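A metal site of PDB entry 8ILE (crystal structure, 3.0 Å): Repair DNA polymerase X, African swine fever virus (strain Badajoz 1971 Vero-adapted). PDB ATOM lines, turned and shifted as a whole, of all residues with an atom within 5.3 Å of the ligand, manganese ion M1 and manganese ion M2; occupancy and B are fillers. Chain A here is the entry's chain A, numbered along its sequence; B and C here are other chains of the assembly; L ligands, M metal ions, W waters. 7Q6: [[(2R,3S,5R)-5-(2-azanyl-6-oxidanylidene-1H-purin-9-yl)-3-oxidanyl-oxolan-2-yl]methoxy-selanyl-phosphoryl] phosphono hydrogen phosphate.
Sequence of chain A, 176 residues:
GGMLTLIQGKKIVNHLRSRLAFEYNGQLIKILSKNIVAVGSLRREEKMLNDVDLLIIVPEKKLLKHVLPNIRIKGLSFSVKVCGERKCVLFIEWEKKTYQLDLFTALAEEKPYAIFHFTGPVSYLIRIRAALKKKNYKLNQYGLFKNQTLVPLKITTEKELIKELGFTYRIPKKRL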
ATOM      1  N   GLY A  40      10.132  20.921  23.865  1.00  0.00           N
ATOM      2  CA  GLY A  40       9.057  20.241  24.593  1.00  0.00           C
ATOM      3  C   GLY A  40       8.275  21.154  25.530  1.00  0.00           C
ATOM      4  O   GLY A  40       8.288  22.382  25.386  1.00  0.00           O
ATOM      5  N   SER A  41       7.644  20.540  26.542  1.00  0.00           N
ATOM      6  CA  SER A  41       6.785  21.256  27.495  1.00  0.00           C
ATOM      7  C   SER A  41       7.450  22.486  28.138  1.00  0.00           C
ATOM      8  O   SER A  41       6.751  23.424  28.482  1.00  0.00           O
ATOM      9  CB  SER A  41       6.236  20.315  28.591  1.00  0.00           C
ATOM     10  OG  SER A  41       7.266  19.546  29.202  1.00  0.00           O
ATOM     11  N   ARG A  44       7.238  25.421  25.665  1.00  0.00           N
ATOM     12  CA  ARG A  44       5.838  25.825  25.599  1.00  0.00           C
ATOM     13  C   ARG A  44       5.370  26.451  26.911  1.00  0.00           C
ATOM     14  O   ARG A  44       4.242  26.950  26.995  1.00  0.00           O
ATOM     15  CB  ARG A  44       4.971  24.622  25.234  1.00  0.00           C
ATOM     16  CG  ARG A  44       5.354  23.978  23.909  1.00  0.00           C
ATOM     17  CD  ARG A  44       4.200  23.192  23.323  1.00  0.00           C
ATOM     18  NE  ARG A  44       3.737  22.181  24.274  1.00  0.00           N
ATOM     19  CZ  ARG A  44       4.314  21.001  24.499  1.00  0.00           C
ATOM     20  NH1 ARG A  44       5.414  20.625  23.844  1.00  0.00           N
ATOM     21  NH2 ARG A  44       3.792  20.178  25.404  1.00  0.00           N
ATOM     22  N   GLU A  46       4.647  25.277  30.008  1.00  0.00           N
ATOM     23  CA  GLU A  46       3.661  24.593  30.830  1.00  0.00           C
ATOM     24  C   GLU A  46       4.084  24.789  32.274  1.00  0.00           C
ATOM     25  O   GLU A  46       5.279  24.809  32.569  1.00  0.00           O
ATOM     26  CB  GLU A  46       3.656  23.106  30.472  1.00  0.00           C
ATOM     27  CG  GLU A  46       3.340  22.873  28.977  1.00  0.00           C
ATOM     28  CD  GLU A  46       2.201  21.884  28.724  1.00  0.00           C
ATOM     29  OE1 GLU A  46       1.495  22.059  27.700  1.00  0.00           O
ATOM     30  OE2 GLU A  46       2.029  20.935  29.514  1.00  0.00           O
ATOM     31  N   MET A  48       3.794  22.690  34.665  1.00  0.00           N
ATOM     32  CA  MET A  48       4.424  21.439  35.100  1.00  0.00           C
ATOM     33  C   MET A  48       5.005  20.618  33.935  1.00  0.00           C
ATOM     34  O   MET A  48       4.360  20.454  32.890  1.00  0.00           O
ATOM     35  CB  MET A  48       3.408  20.590  35.850  1.00  0.00           C
ATOM     36  CG  MET A  48       3.959  19.950  37.106  1.00  0.00           C
ATOM     37  SD  MET A  48       4.292  21.183  38.385  1.00  0.00           S
ATOM     38  CE  MET A  48       4.943  20.155  39.698  1.00  0.00           C
ATOM     39  N   LEU A  49       6.227  20.120  34.130  1.00  0.00           N
ATOM     40  CA  LEU A  49       6.949  19.306  33.138  1.00  0.00           C
ATOM     41  C   LEU A  49       7.167  17.876  33.659  1.00  0.00           C
ATOM     42  O   LEU A  49       7.275  17.675  34.875  1.00  0.00           O
ATOM     43  CB  LEU A  49       8.313  19.925  32.835  1.00  0.00           C
ATOM     44  CG  LEU A  49       8.420  21.437  32.701  1.00  0.00           C
ATOM     45  CD1 LEU A  49       9.879  21.822  32.478  1.00  0.00           C
ATOM     46  CD2 LEU A  49       7.551  21.966  31.567  1.00  0.00           C
ATOM     47  N   ASN A  50       7.254  16.916  32.738  1.00  0.00           N
ATOM     48  CA  ASN A  50       7.637  15.531  33.050  1.00  0.00           C
ATOM     49  C   ASN A  50       9.128  15.296  32.940  1.00  0.00           C
ATOM     50  O   ASN A  50       9.693  14.472  33.663  1.00  0.00           O
ATOM     51  CB  ASN A  50       6.921  14.542  32.148  1.00  0.00           C
ATOM     52  CG  ASN A  50       5.446  14.485  32.415  1.00  0.00           C
ATOM     53  OD1 ASN A  50       4.645  15.050  31.670  1.00  0.00           O
ATOM     54  ND2 ASN A  50       5.074  13.829  33.516  1.00  0.00           N
ATOM     55  N   ASP A  51       9.749  15.993  31.995  1.00  0.00           N
ATOM     56  CA  ASP A  51      11.191  15.900  31.781  1.00  0.00           C
ATOM     57  C   ASP A  51      11.673  17.175  31.112  1.00  0.00           C
ATOM     58  O   ASP A  51      10.869  18.030  30.745  1.00  0.00           O
ATOM     59  CB  ASP A  51      11.525  14.691  30.909  1.00  0.00           C
ATOM     60  CG  ASP A  51      10.846  14.722  29.540  1.00  0.00           C
ATOM     61  OD1 ASP A  51      10.048  15.624  29.260  1.00  0.00           O
ATOM     62  OD2 ASP A  51      11.102  13.808  28.745  1.00  0.00           O
ATOM     63  N   VAL A  52      12.989  17.294  31.006  1.00  0.00           N
ATOM     64  CA  VAL A  52      13.585  18.390  30.268  1.00  0.00           C
ATOM     65  C   VAL A  52      14.033  17.810  28.950  1.00  0.00           C
ATOM     66  O   VAL A  52      14.773  16.821  28.920  1.00  0.00           O
ATOM     67  CB  VAL A  52      14.774  18.984  31.027  1.00  0.00           C
ATOM     68  CG1 VAL A  52      15.452  20.060  30.194  1.00  0.00           C
ATOM     69  CG2 VAL A  52      14.304  19.546  32.361  1.00  0.00           C
ATOM     70  N   ASP A  53      13.582  18.427  27.862  1.00  0.00           N
ATOM     71  CA  ASP A  53      13.923  18.003  26.502  1.00  0.00           C
ATOM     72  C   ASP A  53      14.870  19.028  25.900  1.00  0.00           C
ATOM     73  O   ASP A  53      14.480  20.191  25.758  1.00  0.00           O
ATOM     74  CB  ASP A  53      12.649  17.923  25.664  1.00  0.00           C
ATOM     75  CG  ASP A  53      11.630  16.976  26.263  1.00  0.00           C
ATOM     76  OD1 ASP A  53      11.729  15.757  26.015  1.00  0.00           O
ATOM     77  OD2 ASP A  53      10.726  17.455  26.972  1.00  0.00           O
ATOM     78  N   GLN A 100      14.298  12.884  34.348  1.00  0.00           N
ATOM     79  CA  GLN A 100      14.611  12.470  32.993  1.00  0.00           C
ATOM     80  C   GLN A 100      15.060  13.667  32.163  1.00  0.00           C
ATOM     81  O   GLN A 100      14.465  14.733  32.221  1.00  0.00           O
ATOM     82  CB  GLN A 100      13.392  11.812  32.341  1.00  0.00           C
ATOM     83  CG  GLN A 100      13.619  11.307  30.911  1.00  0.00           C
ATOM     84  CD  GLN A 100      12.488  10.420  30.403  1.00  0.00           C
ATOM     85  OE1 GLN A 100      11.736   9.833  31.189  1.00  0.00           O
ATOM     86  NE2 GLN A 100      12.369  10.317  29.081  1.00  0.00           N
ATOM     87  N   ASP A 102      16.000  14.276  28.135  1.00  0.00           N
ATOM     88  CA  ASP A 102      16.074  13.757  26.767  1.00  0.00           C
ATOM     89  C   ASP A 102      16.852  14.699  25.838  1.00  0.00           C
ATOM     90  O   ASP A 102      16.480  15.855  25.669  1.00  0.00           O
ATOM     91  CB  ASP A 102      14.672  13.514  26.211  1.00  0.00           C
ATOM     92  CG  ASP A 102      13.902  12.469  26.996  1.00  0.00           C
ATOM     93  OD1 ASP A 102      14.551  11.642  27.672  1.00  0.00           O
ATOM     94  OD2 ASP A 102      12.659  12.471  26.940  1.00  0.00           O
ATOM     95  N   PHE A 104      18.290  15.420  22.018  1.00  0.00           N
ATOM     96  CA  PHE A 104      18.181  15.143  20.590  1.00  0.00           C
ATOM     97  C   PHE A 104      19.223  15.969  19.829  1.00  0.00           C
ATOM     98  O   PHE A 104      19.752  16.950  20.366  1.00  0.00           O
ATOM     99  CB  PHE A 104      16.783  15.504  20.102  1.00  0.00           C
ATOM    100  CG  PHE A 104      15.692  15.040  21.024  1.00  0.00           C
ATOM    101  CD1 PHE A 104      15.203  13.753  20.954  1.00  0.00           C
ATOM    102  CD2 PHE A 104      15.153  15.907  21.978  1.00  0.00           C
ATOM    103  CE1 PHE A 104      14.199  13.330  21.815  1.00  0.00           C
ATOM    104  CE2 PHE A 104      14.156  15.488  22.846  1.00  0.00           C
ATOM    105  CZ  PHE A 104      13.674  14.201  22.754  1.00  0.00           C
ATOM    106  N   HIS A 117       9.527  20.593  15.174  1.00  0.00           N
ATOM    107  CA  HIS A 117       9.134  19.211  15.565  1.00  0.00           C
ATOM    108  C   HIS A 117       9.165  18.981  17.076  1.00  0.00           C
ATOM    109  O   HIS A 117       8.157  18.653  17.669  1.00  0.00           O
ATOM    110  CB  HIS A 117      10.053  18.182  14.887  1.00  0.00           C
ATOM    111  CG  HIS A 117       9.959  16.800  15.469  1.00  0.00           C
ATOM    112  ND1 HIS A 117       8.995  15.893  15.094  1.00  0.00           N
ATOM    113  CD2 HIS A 117      10.742  16.148  16.367  1.00  0.00           C
ATOM    114  CE1 HIS A 117       9.175  14.760  15.742  1.00  0.00           C
ATOM    115  NE2 HIS A 117      10.225  14.890  16.527  1.00  0.00           N
ATOM    116  N   PHE A 118      10.340  19.165  17.686  1.00  0.00           N
ATOM    117  CA  PHE A 118      10.523  18.913  19.109  1.00  0.00           C
ATOM    118  C   PHE A 118       9.845  19.905  20.052  1.00  0.00           C
ATOM    119  O   PHE A 118       9.734  19.639  21.244  1.00  0.00           O
ATOM    120  CB  PHE A 118      12.021  18.842  19.463  1.00  0.00           C
ATOM    121  CG  PHE A 118      12.683  17.587  19.001  1.00  0.00           C
ATOM    122  CD1 PHE A 118      12.332  16.353  19.553  1.00  0.00           C
ATOM    123  CD2 PHE A 118      13.651  17.614  18.002  1.00  0.00           C
ATOM    124  CE1 PHE A 118      12.927  15.183  19.123  1.00  0.00           C
ATOM    125  CE2 PHE A 118      14.251  16.435  17.573  1.00  0.00           C
ATOM    126  CZ  PHE A 118      13.892  15.222  18.136  1.00  0.00           C
ATOM    127  N   THR A 119       9.403  21.051  19.526  1.00  0.00           N
ATOM    128  CA  THR A 119       8.678  22.018  20.350  1.00  0.00           C
ATOM    129  C   THR A 119       7.284  21.508  20.667  1.00  0.00           C
ATOM    130  O   THR A 119       6.808  21.688  21.784  1.00  0.00           O
ATOM    131  CB  THR A 119       8.618  23.410  19.686  1.00  0.00           C
ATOM    132  OG1 THR A 119       9.943  23.969  19.732  1.00  0.00           O
ATOM    133  CG2 THR A 119       7.626  24.346  20.410  1.00  0.00           C
ATOM    134  N   GLY A 120       6.647  20.884  19.686  1.00  0.00           N
ATOM    135  CA  GLY A 120       5.347  20.269  19.897  1.00  0.00           C
ATOM    136  C   GLY A 120       4.283  21.343  20.054  1.00  0.00           C
ATOM    137  O   GLY A 120       4.489  22.453  19.543  1.00  0.00           O
ATOM    138  N   PRO A 121       3.158  21.061  20.718  1.00  0.00           N
ATOM    139  CA  PRO A 121       2.807  19.733  21.217  1.00  0.00           C
ATOM    140  C   PRO A 121       2.406  18.797  20.093  1.00  0.00           C
ATOM    141  O   PRO A 121       2.300  19.217  18.949  1.00  0.00           O
ATOM    142  CB  PRO A 121       1.608  20.018  22.103  1.00  0.00           C
ATOM    143  CG  PRO A 121       0.912  21.128  21.392  1.00  0.00           C
ATOM    144  CD  PRO A 121       1.993  21.966  20.765  1.00  0.00           C
ATOM    145  N   VAL A 122       2.132  17.549  20.448  1.00  0.00           N
ATOM    146  CA  VAL A 122       1.919  16.492  19.449  1.00  0.00           C
ATOM    147  C   VAL A 122       0.669  16.787  18.636  1.00  0.00           C
ATOM    148  O   VAL A 122       0.713  16.778  17.406  1.00  0.00           O
ATOM    149  CB  VAL A 122       1.814  15.108  20.130  1.00  0.00           C
ATOM    150  CG1 VAL A 122       1.443  14.024  19.117  1.00  0.00           C
ATOM    151  CG2 VAL A 122       3.136  14.759  20.800  1.00  0.00           C
ATOM    152  N   LEU A 125       1.303  19.202  15.914  1.00  0.00           N
ATOM    153  CA  LEU A 125       2.115  18.553  14.881  1.00  0.00           C
ATOM    154  C   LEU A 125       1.293  17.646  13.946  1.00  0.00           C
ATOM    155  O   LEU A 125       1.584  17.583  12.747  1.00  0.00           O
ATOM    156  CB  LEU A 125       3.242  17.739  15.498  1.00  0.00           C
ATOM    157  CG  LEU A 125       4.365  18.517  16.205  1.00  0.00           C
ATOM    158  CD1 LEU A 125       5.187  17.593  17.081  1.00  0.00           C
ATOM    159  CD2 LEU A 125       5.257  19.223  15.193  1.00  0.00           C
ATOM    160  O5'  DC B   1      -1.236  10.972  11.189  1.00  0.00           O
ATOM    161  C5'  DC B   1      -1.285  12.202  10.425  1.00  0.00           C
ATOM    162  C4'  DC B   1       0.085  12.847  10.382  1.00  0.00           C
ATOM    163  O4'  DC B   1       0.540  13.120  11.724  1.00  0.00           O
ATOM    164  C3'  DC B   1       1.167  12.009   9.698  1.00  0.00           C
ATOM    165  O3'  DC B   1       1.932  12.805   8.787  1.00  0.00           O
ATOM    166  C2'  DC B   1       2.002  11.491  10.859  1.00  0.00           C
ATOM    167  C1'  DC B   1       1.830  12.554  11.922  1.00  0.00           C
ATOM    168  N1   DC B   1       1.872  12.015  13.293  1.00  0.00           N
ATOM    169  C2   DC B   1       3.042  12.172  14.056  1.00  0.00           C
ATOM    170  O2   DC B   1       4.003  12.778  13.563  1.00  0.00           O
ATOM    171  N3   DC B   1       3.090  11.665  15.316  1.00  0.00           N
ATOM    172  C4   DC B   1       2.031  11.016  15.805  1.00  0.00           C
ATOM    173  N4   DC B   1       2.120  10.536  17.056  1.00  0.00           N
ATOM    174  C5   DC B   1       0.837  10.827  15.054  1.00  0.00           C
ATOM    175  C6   DC B   1       0.806  11.333  13.808  1.00  0.00           C
ATOM    176  P    DT B   2       2.900  12.110   7.720  1.00  0.00           P
ATOM    177  OP1  DT B   2       3.212  13.106   6.655  1.00  0.00           O
ATOM    178  OP2  DT B   2       2.329  10.793   7.359  1.00  0.00           O
ATOM    179  O5'  DT B   2       4.220  11.815   8.554  1.00  0.00           O
ATOM    180  C5'  DT B   2       4.992  12.866   9.165  1.00  0.00           C
ATOM    181  C4'  DT B   2       6.093  12.255   9.992  1.00  0.00           C
ATOM    182  O4'  DT B   2       5.565  11.817  11.256  1.00  0.00           O
ATOM    183  C3'  DT B   2       6.752  11.011   9.365  1.00  0.00           C
ATOM    184  O3'  DT B   2       8.066  11.298   8.874  1.00  0.00           O
ATOM    185  C2'  DT B   2       6.754   9.971  10.483  1.00  0.00           C
ATOM    186  C1'  DT B   2       6.382  10.761  11.719  1.00  0.00           C
ATOM    187  N1   DT B   2       5.621  10.003  12.740  1.00  0.00           N
ATOM    188  C2   DT B   2       6.122   9.948  14.024  1.00  0.00           C
ATOM    189  O2   DT B   2       7.146  10.514  14.363  1.00  0.00           O
ATOM    190  N3   DT B   2       5.366   9.219  14.906  1.00  0.00           N
ATOM    191  C4   DT B   2       4.188   8.550  14.634  1.00  0.00           C
ATOM    192  O4   DT B   2       3.615   7.935  15.533  1.00  0.00           O
ATOM    193  C5   DT B   2       3.722   8.642  13.268  1.00  0.00           C
ATOM    194  C7   DT B   2       2.460   7.945  12.884  1.00  0.00           C
ATOM    195  C6   DT B   2       4.455   9.353  12.402  1.00  0.00           C
ATOM    196  P    DA C   9      11.756   7.600  25.856  1.00  0.00           P
ATOM    197  OP1  DA C   9      13.139   7.061  25.952  1.00  0.00           O
ATOM    198  OP2  DA C   9      11.106   8.211  27.067  1.00  0.00           O
ATOM    199  O5'  DA C   9      11.689   8.680  24.675  1.00  0.00           O
ATOM    200  C5'  DA C   9      10.788   9.813  24.749  1.00  0.00           C
ATOM    201  C4'  DA C   9      11.057  10.759  23.604  1.00  0.00           C
ATOM    202  O4'  DA C   9      10.877  10.067  22.346  1.00  0.00           O
ATOM    203  C3'  DA C   9      10.132  11.973  23.539  1.00  0.00           C
ATOM    204  C2'  DA C   9      10.099  12.281  22.047  1.00  0.00           C
ATOM    205  C1'  DA C   9      10.199  10.903  21.413  1.00  0.00           C
ATOM    206  N9   DA C   9       8.923  10.261  21.086  1.00  0.00           N
ATOM    207  C8   DA C   9       8.064   9.628  21.955  1.00  0.00           C
ATOM    208  N7   DA C   9       7.018   9.107  21.360  1.00  0.00           N
ATOM    209  C5   DA C   9       7.206   9.399  20.023  1.00  0.00           C
ATOM    210  C6   DA C   9       6.440   9.115  18.877  1.00  0.00           C
ATOM    211  N6   DA C   9       5.282   8.461  18.902  1.00  0.00           N
ATOM    212  N1   DA C   9       6.911   9.549  17.684  1.00  0.00           N
ATOM    213  C2   DA C   9       8.078  10.217  17.657  1.00  0.00           C
ATOM    214  N3   DA C   9       8.879  10.554  18.669  1.00  0.00           N
ATOM    215  C4   DA C   9       8.382  10.105  19.835  1.00  0.00           C
HETATM  216  O3G 7Q6 L   1       5.084  15.246  28.924  1.00  0.00           O
HETATM  217  PG  7Q6 L   1       5.964  16.468  28.796  1.00  0.00           P
HETATM  218  O1G 7Q6 L   1       7.395  16.033  28.688  1.00  0.00           O
HETATM  219  O2G 7Q6 L   1       5.820  17.404  29.975  1.00  0.00           O
HETATM  220  O3B 7Q6 L   1       5.481  17.191  27.445  1.00  0.00           O
HETATM  221  PB  7Q6 L   1       6.270  17.047  26.058  1.00  0.00           P
HETATM  222  O1B 7Q6 L   1       5.498  17.902  25.085  1.00  0.00           O
HETATM  223  O2B 7Q6 L   1       7.628  17.636  26.307  1.00  0.00           O
HETATM  224  O3A 7Q6 L   1       6.244  15.506  25.527  1.00  0.00           O
HETATM  225  PA  7Q6 L   1       7.430  14.486  25.123  1.00  0.00           P
HETATM  226 SEA  7Q6 L   1       8.867  14.631  26.334  1.00  0.00          SE
HETATM  227  O1A 7Q6 L   1       6.996  12.931  25.086  1.00  0.00           O
HETATM  228  O5' 7Q6 L   1       8.143  14.916  23.764  1.00  0.00           O
HETATM  229  C5' 7Q6 L   1       9.017  16.025  23.628  1.00  0.00           C
HETATM  230  C4' 7Q6 L   1       8.858  16.506  22.206  1.00  0.00           C
HETATM  231  O4' 7Q6 L   1       9.051  15.426  21.280  1.00  0.00           O
HETATM  232  C3' 7Q6 L   1       7.466  17.054  21.951  1.00  0.00           C
HETATM  233  O3' 7Q6 L   1       7.405  18.456  22.213  1.00  0.00           O
HETATM  234  C2' 7Q6 L   1       7.222  16.747  20.489  1.00  0.00           C
HETATM  235  C1' 7Q6 L   1       8.087  15.518  20.220  1.00  0.00           C
HETATM  236  N9  7Q6 L   1       7.160  14.377  20.202  1.00  0.00           N
HETATM  237  C4  7Q6 L   1       6.548  13.938  19.127  1.00  0.00           C
HETATM  238  N3  7Q6 L   1       6.570  14.259  17.812  1.00  0.00           N
HETATM  239  C2  7Q6 L   1       5.795  13.569  16.951  1.00  0.00           C
HETATM  240  N2  7Q6 L   1       5.813  13.902  15.649  1.00  0.00           N
HETATM  241  N1  7Q6 L   1       5.008  12.534  17.364  1.00  0.00           N
HETATM  242  C8  7Q6 L   1       6.747  13.654  21.260  1.00  0.00           C
HETATM  243  N7  7Q6 L   1       5.869  12.709  20.898  1.00  0.00           N
HETATM  244  C5  7Q6 L   1       5.705  12.818  19.578  1.00  0.00           C
HETATM  245  C6  7Q6 L   1       4.950  12.152  18.671  1.00  0.00           C
HETATM  246  O6  7Q6 L   1       4.232  11.223  19.080  1.00  0.00           O
HETATM  247 MN    MN M   1      10.875  13.624  26.655  1.00  0.00          MN
HETATM  248 MN    MN M   2       9.065  16.726  27.761  1.00  0.00          MN
HETATM  249  O   HOH W   1       9.175  18.408  28.846  1.00  0.00           O
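An oxygen (O2B) of the ligand lies close to the backbone NH (N) of Ser 41, 2.9 Å away. The side-chain hydroxyl (OG) of Ser 41 is in hydrogen-bond range of an oxygen (O2G) of the ligand. O of Phe 118 sits at hydrogen-bond distance from O3' of the ligand. An oxygen (O2G) of the ligand is in hydrogen-bond range of the backbone NH of Asn 50 (3.2 Å). The side-chain amide oxygen (OD1) of Asn 50 lies close to an oxygen (O3G) of the ligand, 2.8 Å away. The guanidinium group (NH2) of Arg 44 lies within salt-bridge range of an oxygen (O1B) of the ligand (2.9 Å). N1 of the ligand is in hydrogen-bond range of N3 of DC 1 of chain B. O of Thr 119 lies within hydrogen-bond range of O3' of the ligand (3.3 Å).
The side-chain carboxylate (OD1) of Asp 102 is in hydrogen-bond range of the side-chain amide nitrogen (NE2) of Gln 100 (2.9 Å). The backbone NH of Asp 102 sits at hydrogen-bond distance from the backbone carbonyl oxygen of Val 52 (2.9 Å). The backbone carbonyl oxygen (O) of Ser 41 lies within hydrogen-bond range of the backbone NH (N) of Glu 46, 3.2 Å away. O of Phe 118 sits at hydrogen-bond distance from N of Gly 40. O of Thr 119 is in hydrogen-bond range of NH1 of Arg 44. NH2 of Arg 44 lies within salt-bridge range of OE1 of Glu 46 (3.8 Å). OP2 of DA 9 of chain C is in hydrogen-bond range of NE2 of Gln 100, at 3.2 Å.
N6 of DA 9 of chain C sits close to O6 of the ligand (3.0 Å). Merely in contact with the ligand: Gly 40 (3.4 Å), Leu 49 (3.9 Å), His 117 (3.4 Å), Gly 120 (3.6 Å), Val 122 (3.4 Å), Leu 125 (3.7 Å) and DT 2 of chain B (3.9 Å). Hydrophobic or aromatic side chains that line the ligand: His 117, Phe 118, Val 122 and Leu 125. Of the 23 residues printed, 16 come within 4 Å of the ligand. The nearest printed residue that does not touch the ligand is Asp 102 (4.4 Å).
DA 9 of chain C touches manganese ion M1 (C3' to MN, 3.6 Å).
Ser 41 touches manganese ion M2. Within 4 Å of manganese ion M2: Ser 41, Asp 51 and Asp 53.
Manganese ion M1 is bound by the side-chain carboxylate (OD2) of Asp 51 (2.1 Å), the side-chain carboxylate (OD2) of Asp 102 (2.1 Å), a selenium (SEA) of the ligand (2.3 Å) and the side-chain carboxylate (OD1) of Asp 53 (2.4 Å). Manganese ion M1 has four donor atoms within binding distance.
Manganese ion M2 is bound by OD2 of Asp 53 (2.0 Å), water W1 (2.0 Å), O1G of the ligand (2.0 Å), OD1 of Asp 51 (2.1 Å), O2B of the ligand (2.2 Å) and SEA of the ligand (2.5 Å). Manganese ion M2 has six donor atoms within binding distance.
Water W1 bridges O of Asp 51 (2.6 Å) and N of Ser 41 (3.5 Å).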
